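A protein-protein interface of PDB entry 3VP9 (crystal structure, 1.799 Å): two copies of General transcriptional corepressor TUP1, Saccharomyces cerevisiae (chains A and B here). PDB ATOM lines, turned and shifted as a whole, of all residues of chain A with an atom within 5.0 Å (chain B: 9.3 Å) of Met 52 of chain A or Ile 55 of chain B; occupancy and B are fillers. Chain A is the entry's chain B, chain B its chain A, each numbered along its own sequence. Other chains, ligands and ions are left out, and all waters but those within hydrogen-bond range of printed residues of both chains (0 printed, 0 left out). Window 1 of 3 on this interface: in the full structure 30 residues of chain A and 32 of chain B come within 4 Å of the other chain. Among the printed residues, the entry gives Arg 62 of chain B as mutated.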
ATOM      1  N   GLN A  48      35.294   0.354   2.735  1.00  0.00           N
ATOM      2  CA  GLN A  48      34.021  -0.355   2.577  1.00  0.00           C
ATOM      3  C   GLN A  48      32.960   0.582   2.017  1.00  0.00           C
ATOM      4  O   GLN A  48      32.168   0.193   1.142  1.00  0.00           O
ATOM      5  CB  GLN A  48      33.556  -0.923   3.920  1.00  0.00           C
ATOM      6  CG  GLN A  48      32.790  -2.236   3.841  1.00  0.00           C
ATOM      7  CD  GLN A  48      33.692  -3.463   3.978  1.00  0.00           C
ATOM      8  OE1 GLN A  48      34.065  -3.858   5.088  1.00  0.00           O
ATOM      9  NE2 GLN A  48      34.044  -4.068   2.847  1.00  0.00           N
ATOM     10  N   LEU A  49      32.941   1.814   2.519  1.00  0.00           N
ATOM     11  CA  LEU A  49      31.968   2.803   2.064  1.00  0.00           C
ATOM     12  C   LEU A  49      32.122   3.015   0.568  1.00  0.00           C
ATOM     13  O   LEU A  49      31.133   3.056  -0.167  1.00  0.00           O
ATOM     14  CB  LEU A  49      32.171   4.134   2.789  1.00  0.00           C
ATOM     15  CG  LEU A  49      30.916   4.977   3.027  1.00  0.00           C
ATOM     16  CD1 LEU A  49      30.175   4.477   4.263  1.00  0.00           C
ATOM     17  CD2 LEU A  49      31.253   6.452   3.181  1.00  0.00           C
ATOM     18  N   ALA A  50      33.369   3.150   0.125  1.00  0.00           N
ATOM     19  CA  ALA A  50      33.667   3.390  -1.282  1.00  0.00           C
ATOM     20  C   ALA A  50      33.245   2.198  -2.149  1.00  0.00           C
ATOM     21  O   ALA A  50      32.684   2.375  -3.239  1.00  0.00           O
ATOM     22  CB  ALA A  50      35.133   3.690  -1.471  1.00  0.00           C
ATOM     23  N   GLU A  51      33.529   0.989  -1.665  1.00  0.00           N
ATOM     24  CA  GLU A  51      33.125  -0.220  -2.380  1.00  0.00           C
ATOM     25  C   GLU A  51      31.601  -0.267  -2.515  1.00  0.00           C
ATOM     26  O   GLU A  51      31.076  -0.547  -3.592  1.00  0.00           O
ATOM     27  CB  GLU A  51      33.684  -1.476  -1.703  1.00  0.00           C
ATOM     28  CG  GLU A  51      35.221  -1.525  -1.701  1.00  0.00           C
ATOM     29  CD  GLU A  51      35.797  -2.856  -1.241  1.00  0.00           C
ATOM     30  OE1 GLU A  51      35.084  -3.888  -1.320  1.00  0.00           O
ATOM     31  OE2 GLU A  51      36.988  -2.880  -0.824  1.00  0.00           O
ATOM     32  N   MET A  52      30.896   0.029  -1.430  1.00  0.00           N
ATOM     33  CA  MET A  52      29.436   0.082  -1.470  1.00  0.00           C
ATOM     34  C   MET A  52      28.927   1.144  -2.455  1.00  0.00           C
ATOM     35  O   MET A  52      27.892   0.957  -3.084  1.00  0.00           O
ATOM     36  CB  MET A  52      28.865   0.337  -0.068  1.00  0.00           C
ATOM     37  CG  MET A  52      29.002  -0.847   0.877  1.00  0.00           C
ATOM     38  SD  MET A  52      28.139  -2.307   0.232  1.00  0.00           S
ATOM     39  CE  MET A  52      27.551  -3.053   1.755  1.00  0.00           C
ATOM     40  N   GLN A  53      29.634   2.266  -2.580  1.00  0.00           N
ATOM     41  CA  GLN A  53      29.217   3.315  -3.527  1.00  0.00           C
ATOM     42  C   GLN A  53      29.391   2.833  -4.963  1.00  0.00           C
ATOM     43  O   GLN A  53      28.577   3.142  -5.846  1.00  0.00           O
ATOM     44  CB  GLN A  53      29.993   4.628  -3.306  1.00  0.00           C
ATOM     45  CG  GLN A  53      29.636   5.401  -2.048  1.00  0.00           C
ATOM     46  CD  GLN A  53      30.708   6.438  -1.674  1.00  0.00           C
ATOM     47  OE1 GLN A  53      31.861   6.347  -2.107  1.00  0.00           O
ATOM     48  NE2 GLN A  53      30.324   7.422  -0.865  1.00  0.00           N
ATOM     49  N   GLN A  54      30.451   2.064  -5.187  1.00  0.00           N
ATOM     50  CA  GLN A  54      30.691   1.412  -6.474  1.00  0.00           C
ATOM     51  C   GLN A  54      29.570   0.448  -6.839  1.00  0.00           C
ATOM     52  O   GLN A  54      29.100   0.432  -7.971  1.00  0.00           O
ATOM     53  CB  GLN A  54      32.019   0.670  -6.459  1.00  0.00           C
ATOM     54  CG  GLN A  54      33.243   1.580  -6.351  1.00  0.00           C
ATOM     55  CD  GLN A  54      34.537   0.785  -6.197  1.00  0.00           C
ATOM     56  OE1 GLN A  54      34.538  -0.315  -5.648  1.00  0.00           O
ATOM     57  NE2 GLN A  54      35.644   1.343  -6.688  1.00  0.00           N
ATOM     58  N   ILE A  55      29.166  -0.367  -5.876  1.00  0.00           N
ATOM     59  CA  ILE A  55      28.087  -1.314  -6.078  1.00  0.00           C
ATOM     60  C   ILE A  55      26.782  -0.580  -6.379  1.00  0.00           C
ATOM     61  O   ILE A  55      26.072  -0.950  -7.292  1.00  0.00           O
ATOM     62  CB  ILE A  55      27.916  -2.208  -4.869  1.00  0.00           C
ATOM     63  CG1 ILE A  55      29.090  -3.195  -4.801  1.00  0.00           C
ATOM     64  CG2 ILE A  55      26.602  -3.015  -4.955  1.00  0.00           C
ATOM     65  CD1 ILE A  55      29.242  -3.850  -3.457  1.00  0.00           C
ATOM     66  N   ARG A  56      26.497   0.463  -5.607  1.00  0.00           N
ATOM     67  CA  ARG A  56      25.306   1.291  -5.803  1.00  0.00           C
ATOM     68  C   ARG A  56      25.275   1.884  -7.209  1.00  0.00           C
ATOM     69  O   ARG A  56      24.260   1.823  -7.894  1.00  0.00           O
ATOM     70  CB  ARG A  56      25.270   2.417  -4.765  1.00  0.00           C
ATOM     71  CG  ARG A  56      24.167   3.478  -5.001  1.00  0.00           C
ATOM     72  CD  ARG A  56      24.187   4.549  -3.921  1.00  0.00           C
ATOM     73  NE  ARG A  56      23.204   5.627  -4.117  1.00  0.00           N
ATOM     74  CZ  ARG A  56      23.500   6.811  -4.642  1.00  0.00           C
ATOM     75  NH1 ARG A  56      24.748   7.050  -5.031  1.00  0.00           N
ATOM     76  NH2 ARG A  56      22.564   7.750  -4.771  1.00  0.00           N
ATOM     77  N   GLN B  47      31.757  -9.789   9.494  1.00  0.00           N
ATOM     78  CA  GLN B  47      30.329  -9.576   9.341  1.00  0.00           C
ATOM     79  C   GLN B  47      30.060  -8.699   8.126  1.00  0.00           C
ATOM     80  O   GLN B  47      29.284  -9.067   7.235  1.00  0.00           O
ATOM     81  CB  GLN B  47      29.765  -8.913  10.595  1.00  0.00           C
ATOM     82  CG  GLN B  47      28.278  -9.116  10.785  1.00  0.00           C
ATOM     83  CD  GLN B  47      27.969  -9.941  12.019  1.00  0.00           C
ATOM     84  OE1 GLN B  47      27.439  -9.426  13.005  1.00  0.00           O
ATOM     85  NE2 GLN B  47      28.295 -11.228  11.971  1.00  0.00           N
ATOM     86  N   GLN B  48      30.723  -7.547   8.086  1.00  0.00           N
ATOM     87  CA  GLN B  48      30.543  -6.593   6.995  1.00  0.00           C
ATOM     88  C   GLN B  48      30.948  -7.167   5.644  1.00  0.00           C
ATOM     89  O   GLN B  48      30.312  -6.878   4.635  1.00  0.00           O
ATOM     90  CB  GLN B  48      31.332  -5.308   7.262  1.00  0.00           C
ATOM     91  CG  GLN B  48      30.469  -4.149   7.725  1.00  0.00           C
ATOM     92  CD  GLN B  48      29.831  -4.405   9.073  1.00  0.00           C
ATOM     93  OE1 GLN B  48      28.807  -5.084   9.171  1.00  0.00           O
ATOM     94  NE2 GLN B  48      30.441  -3.863  10.125  1.00  0.00           N
ATOM     95  N   LEU B  49      32.018  -7.954   5.630  1.00  0.00           N
ATOM     96  CA  LEU B  49      32.509  -8.539   4.388  1.00  0.00           C
ATOM     97  C   LEU B  49      31.489  -9.524   3.858  1.00  0.00           C
ATOM     98  O   LEU B  49      31.180  -9.529   2.668  1.00  0.00           O
ATOM     99  CB  LEU B  49      33.836  -9.248   4.623  1.00  0.00           C
ATOM    100  CG  LEU B  49      35.010  -8.293   4.831  1.00  0.00           C
ATOM    101  CD1 LEU B  49      36.168  -9.011   5.501  1.00  0.00           C
ATOM    102  CD2 LEU B  49      35.431  -7.666   3.511  1.00  0.00           C
ATOM    103  N   ALA B  50      30.978 -10.371   4.746  1.00  0.00           N
ATOM    104  CA  ALA B  50      29.982 -11.362   4.347  1.00  0.00           C
ATOM    105  C   ALA B  50      28.718 -10.660   3.854  1.00  0.00           C
ATOM    106  O   ALA B  50      28.107 -11.072   2.871  1.00  0.00           O
ATOM    107  CB  ALA B  50      29.668 -12.297   5.501  1.00  0.00           C
ATOM    108  N   GLU B  51      28.326  -9.596   4.543  1.00  0.00           N
ATOM    109  CA  GLU B  51      27.134  -8.870   4.150  1.00  0.00           C
ATOM    110  C   GLU B  51      27.331  -8.253   2.776  1.00  0.00           C
ATOM    111  O   GLU B  51      26.429  -8.288   1.948  1.00  0.00           O
ATOM    112  CB  GLU B  51      26.766  -7.803   5.189  1.00  0.00           C
ATOM    113  CG  GLU B  51      26.233  -8.387   6.488  1.00  0.00           C
ATOM    114  CD  GLU B  51      26.030  -7.334   7.566  1.00  0.00           C
ATOM    115  OE1 GLU B  51      26.285  -6.134   7.300  1.00  0.00           O
ATOM    116  OE2 GLU B  51      25.616  -7.708   8.682  1.00  0.00           O
ATOM    117  N   MET B  52      28.508  -7.689   2.528  1.00  0.00           N
ATOM    118  CA  MET B  52      28.776  -7.129   1.214  1.00  0.00           C
ATOM    119  C   MET B  52      28.722  -8.206   0.123  1.00  0.00           C
ATOM    120  O   MET B  52      28.192  -7.968  -0.955  1.00  0.00           O
ATOM    121  CB  MET B  52      30.125  -6.395   1.174  1.00  0.00           C
ATOM    122  CG  MET B  52      30.204  -5.461  -0.022  1.00  0.00           C
ATOM    123  SD  MET B  52      31.747  -4.559  -0.118  1.00  0.00           S
ATOM    124  CE  MET B  52      32.886  -5.861   0.130  1.00  0.00           C
ATOM    125  N   GLN B  53      29.293  -9.375   0.385  1.00  0.00           N
ATOM    126  CA  GLN B  53      29.267 -10.437  -0.619  1.00  0.00           C
ATOM    127  C   GLN B  53      27.835 -10.859  -0.913  1.00  0.00           C
ATOM    128  O   GLN B  53      27.478 -11.082  -2.064  1.00  0.00           O
ATOM    129  CB  GLN B  53      30.078 -11.670  -0.214  1.00  0.00           C
ATOM    130  CG  GLN B  53      30.221 -12.669  -1.374  1.00  0.00           C
ATOM    131  CD  GLN B  53      30.907 -12.020  -2.567  1.00  0.00           C
ATOM    132  OE1 GLN B  53      31.968 -11.413  -2.420  1.00  0.00           O
ATOM    133  NE2 GLN B  53      30.295 -12.105  -3.732  1.00  0.00           N
ATOM    134  N   GLN B  54      27.020 -10.973   0.132  1.00  0.00           N
ATOM    135  CA  GLN B  54      25.606 -11.313  -0.056  1.00  0.00           C
ATOM    136  C   GLN B  54      24.913 -10.299  -0.968  1.00  0.00           C
ATOM    137  O   GLN B  54      24.157 -10.675  -1.848  1.00  0.00           O
ATOM    138  CB  GLN B  54      24.898 -11.384   1.291  1.00  0.00           C
ATOM    139  CG  GLN B  54      23.383 -11.438   1.185  1.00  0.00           C
ATOM    140  CD  GLN B  54      22.719 -11.601   2.537  1.00  0.00           C
ATOM    141  OE1 GLN B  54      23.267 -11.188   3.564  1.00  0.00           O
ATOM    142  NE2 GLN B  54      21.536 -12.208   2.548  1.00  0.00           N
ATOM    143  N   ILE B  55      25.171  -9.004  -0.766  1.00  0.00           N
ATOM    144  CA  ILE B  55      24.549  -7.990  -1.612  1.00  0.00           C
ATOM    145  C   ILE B  55      24.946  -8.169  -3.080  1.00  0.00           C
ATOM    146  O   ILE B  55      24.096  -8.105  -3.984  1.00  0.00           O
ATOM    147  CB  ILE B  55      24.930  -6.563  -1.135  1.00  0.00           C
ATOM    148  CG1 ILE B  55      24.255  -6.260   0.210  1.00  0.00           C
ATOM    149  CG2 ILE B  55      24.562  -5.510  -2.185  1.00  0.00           C
ATOM    150  CD1 ILE B  55      24.803  -5.009   0.909  1.00  0.00           C
ATOM    151  N   ARG B  56      26.231  -8.411  -3.318  1.00  0.00           N
ATOM    152  CA  ARG B  56      26.712  -8.612  -4.677  1.00  0.00           C
ATOM    153  C   ARG B  56      26.079  -9.872  -5.292  1.00  0.00           C
ATOM    154  O   ARG B  56      25.698  -9.884  -6.477  1.00  0.00           O
ATOM    155  CB  ARG B  56      28.257  -8.703  -4.668  1.00  0.00           C
ATOM    156  CG  ARG B  56      28.929  -7.412  -4.180  1.00  0.00           C
ATOM    157  CD  ARG B  56      30.468  -7.607  -4.052  1.00  0.00           C
ATOM    158  NE  ARG B  56      31.027  -7.876  -5.372  1.00  0.00           N
ATOM    159  CZ  ARG B  56      31.422  -6.942  -6.226  1.00  0.00           C
ATOM    160  NH1 ARG B  56      31.417  -5.651  -5.876  1.00  0.00           N
ATOM    161  NH2 ARG B  56      31.850  -7.309  -7.423  1.00  0.00           N
ATOM    162  N   ASN B  57      25.994 -10.938  -4.503  1.00  0.00           N
ATOM    163  CA  ASN B  57      25.365 -12.178  -4.960  1.00  0.00           C
ATOM    164  C   ASN B  57      23.940 -11.940  -5.470  1.00  0.00           C
ATOM    165  O   ASN B  57      23.525 -12.496  -6.479  1.00  0.00           O
ATOM    166  CB  ASN B  57      25.335 -13.199  -3.827  1.00  0.00           C
ATOM    167  CG  ASN B  57      26.687 -13.829  -3.578  1.00  0.00           C
ATOM    168  OD1 ASN B  57      27.640 -13.612  -4.333  1.00  0.00           O
ATOM    169  ND2 ASN B  57      26.775 -14.626  -2.524  1.00  0.00           N
ATOM    170  N   THR B  58      23.202 -11.125  -4.737  1.00  0.00           N
ATOM    171  CA  THR B  58      21.816 -10.787  -5.089  1.00  0.00           C
ATOM    172  C   THR B  58      21.753 -10.043  -6.417  1.00  0.00           C
ATOM    173  O   THR B  58      20.846 -10.248  -7.201  1.00  0.00           O
ATOM    174  CB  THR B  58      21.128  -9.982  -3.997  1.00  0.00           C
ATOM    175  OG1 THR B  58      21.025 -10.791  -2.826  1.00  0.00           O
ATOM    176  CG2 THR B  58      19.704  -9.584  -4.437  1.00  0.00           C
ATOM    177  N   VAL B  59      22.746  -9.211  -6.693  1.00  0.00           N
ATOM    178  CA  VAL B  59      22.803  -8.540  -7.985  1.00  0.00           C
ATOM    179  C   VAL B  59      22.904  -9.548  -9.136  1.00  0.00           C
ATOM    180  O   VAL B  59      22.156  -9.452 -10.104  1.00  0.00           O
ATOM    181  CB  VAL B  59      23.939  -7.484  -8.035  1.00  0.00           C
ATOM    182  CG1 VAL B  59      24.053  -6.862  -9.428  1.00  0.00           C
ATOM    183  CG2 VAL B  59      23.674  -6.391  -7.003  1.00  0.00           C
ATOM    184  N   TYR B  60      23.803 -10.526  -9.034  1.00  0.00           N
ATOM    185  CA  TYR B  60      23.887 -11.580 -10.048  1.00  0.00           C
ATOM    186  C   TYR B  60      22.602 -12.375 -10.203  1.00  0.00           C
ATOM    187  O   TYR B  60      22.172 -12.692 -11.322  1.00  0.00           O
ATOM    188  CB  TYR B  60      25.005 -12.566  -9.708  1.00  0.00           C
ATOM    189  CG  TYR B  60      26.383 -11.974  -9.839  1.00  0.00           C
ATOM    190  CD1 TYR B  60      26.920 -11.695 -11.092  1.00  0.00           C
ATOM    191  CD2 TYR B  60      27.149 -11.703  -8.716  1.00  0.00           C
ATOM    192  CE1 TYR B  60      28.201 -11.159 -11.226  1.00  0.00           C
ATOM    193  CE2 TYR B  60      28.433 -11.166  -8.842  1.00  0.00           C
ATOM    194  CZ  TYR B  60      28.948 -10.905 -10.098  1.00  0.00           C
ATOM    195  OH  TYR B  60      30.216 -10.380 -10.236  1.00  0.00           O
ATOM    196  N   GLU B  61      22.003 -12.725  -9.074  1.00  0.00           N
ATOM    197  CA  GLU B  61      20.771 -13.512  -9.086  1.00  0.00           C
ATOM    198  C   GLU B  61      19.676 -12.728  -9.779  1.00  0.00           C
ATOM    199  O   GLU B  61      18.929 -13.254 -10.600  1.00  0.00           O
ATOM    200  CB  GLU B  61      20.370 -13.865  -7.650  1.00  0.00           C
ATOM    201  CG  GLU B  61      21.267 -14.962  -7.071  1.00  0.00           C
ATOM    202  CD  GLU B  61      21.281 -15.015  -5.560  1.00  0.00           C
ATOM    203  OE1 GLU B  61      20.375 -14.431  -4.930  1.00  0.00           O
ATOM    204  OE2 GLU B  61      22.218 -15.628  -4.996  1.00  0.00           O
ATOM    205  N   ARG B  62      19.636 -11.438  -9.487  1.00  0.00           N
ATOM    206  CA  ARG B  62      18.619 -10.587 -10.035  1.00  0.00           C
ATOM    207  C   ARG B  62      18.779 -10.490 -11.544  1.00  0.00           C
ATOM    208  O   ARG B  62      17.794 -10.431 -12.270  1.00  0.00           O
ATOM    209  CB  ARG B  62      18.682  -9.215  -9.383  1.00  0.00           C
ATOM    210  CG  ARG B  62      17.449  -8.394  -9.652  1.00  0.00           C
ATOM    211  CD  ARG B  62      17.477  -7.094  -8.881  1.00  0.00           C
ATOM    212  NE  ARG B  62      16.315  -6.296  -9.261  1.00  0.00           N
ATOM    213  CZ  ARG B  62      16.372  -5.062  -9.726  1.00  0.00           C
ATOM    214  NH1 ARG B  62      15.243  -4.443 -10.060  1.00  0.00           N
ATOM    215  NH2 ARG B  62      17.544  -4.448  -9.828  1.00  0.00           N
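Gln 48 of chain B touches Gln 48 of chain A (CB to OE1, 3.8 Å).
CD2 of Leu 49 of chain B touches NE2 of Gln 48 of chain A (3.9 Å).
SD of Met 52 of chain A touches CG of Met 52 of chain B, at 3.8 Å.
Ile 55 of chain B touches Met 52 of chain A.
CD1 of Ile 55 of chain A touches CG of Met 52 of chain B, at 3.9 Å.
NH1 of Arg 56 of chain B touches CG1 of Ile 55 of chain A (3.5 Å).
Printed residues of chain A that touch a printed residue of chain B: Gln 48, Glu 51, Met 52 and Ile 55.
Hydrophobic or aromatic side chains of chain A that line the printed part of chain B: Met 52 and Ile 55.
The side-chain amide nitrogen (NE2) of Gln 48 of chain A sits close to the side-chain sulfur (SD) of Met 52 of chain B, at 3.8 Å.
The side-chain sulfur (SD) of Met 52 of chain B sits close to the side-chain carboxylate (OE1) of Glu 51 of chain A.
Of the printed residues of chain B, Gln 48 of chain A touches Gln 48 (3.8 Å), Leu 49 (3.9 Å) and Met 52 (3.5 Å).
Met 52 of chain A touches just these residues of chain B: Met 52 and Ile 55.
Of the printed residues of chain A, Gln 48 of chain B touches Gln 48 (3.8 Å).
Of the printed residues of chain A, Leu 49 of chain B touches Gln 48 (3.9 Å).
Printed residues of chain A within 4 Å of Met 52 of chain B: Gln 48 (3.5 Å), Glu 51 (3.3 Å), Met 52 (3.8 Å) and Ile 55 (3.9 Å).
Of chain A, only Met 52 comes within 4 Å of Ile 55 of chain B.
Tyr 60 of chain B touches none of the printed residues of chain A.
Arg 62 of chain B touches none of the printed residues of chain A.
The side-chain carboxylate of Glu 51 of chain B sits close to the side-chain amide oxygen of Gln 48 of chain B, at 3.3 Å.
Gln 48 of chain A touches its own counterpart, Gln 48 of chain B.
Gln 48 of chain A touches Leu 49 of chain B, but with the chains exchanged Leu 49 of chain A does not touch Gln 48 of chain B (8.3 Å).
Gln 48 of chain A touches Met 52 of chain B, but with the chains exchanged Met 52 of chain A does not touch Gln 48 of chain B (5.5 Å).
Glu 51 of chain A touches Met 52 of chain B, but with the chains exchanged Met 52 of chain A does not touch Glu 51 of chain B (5.3 Å).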
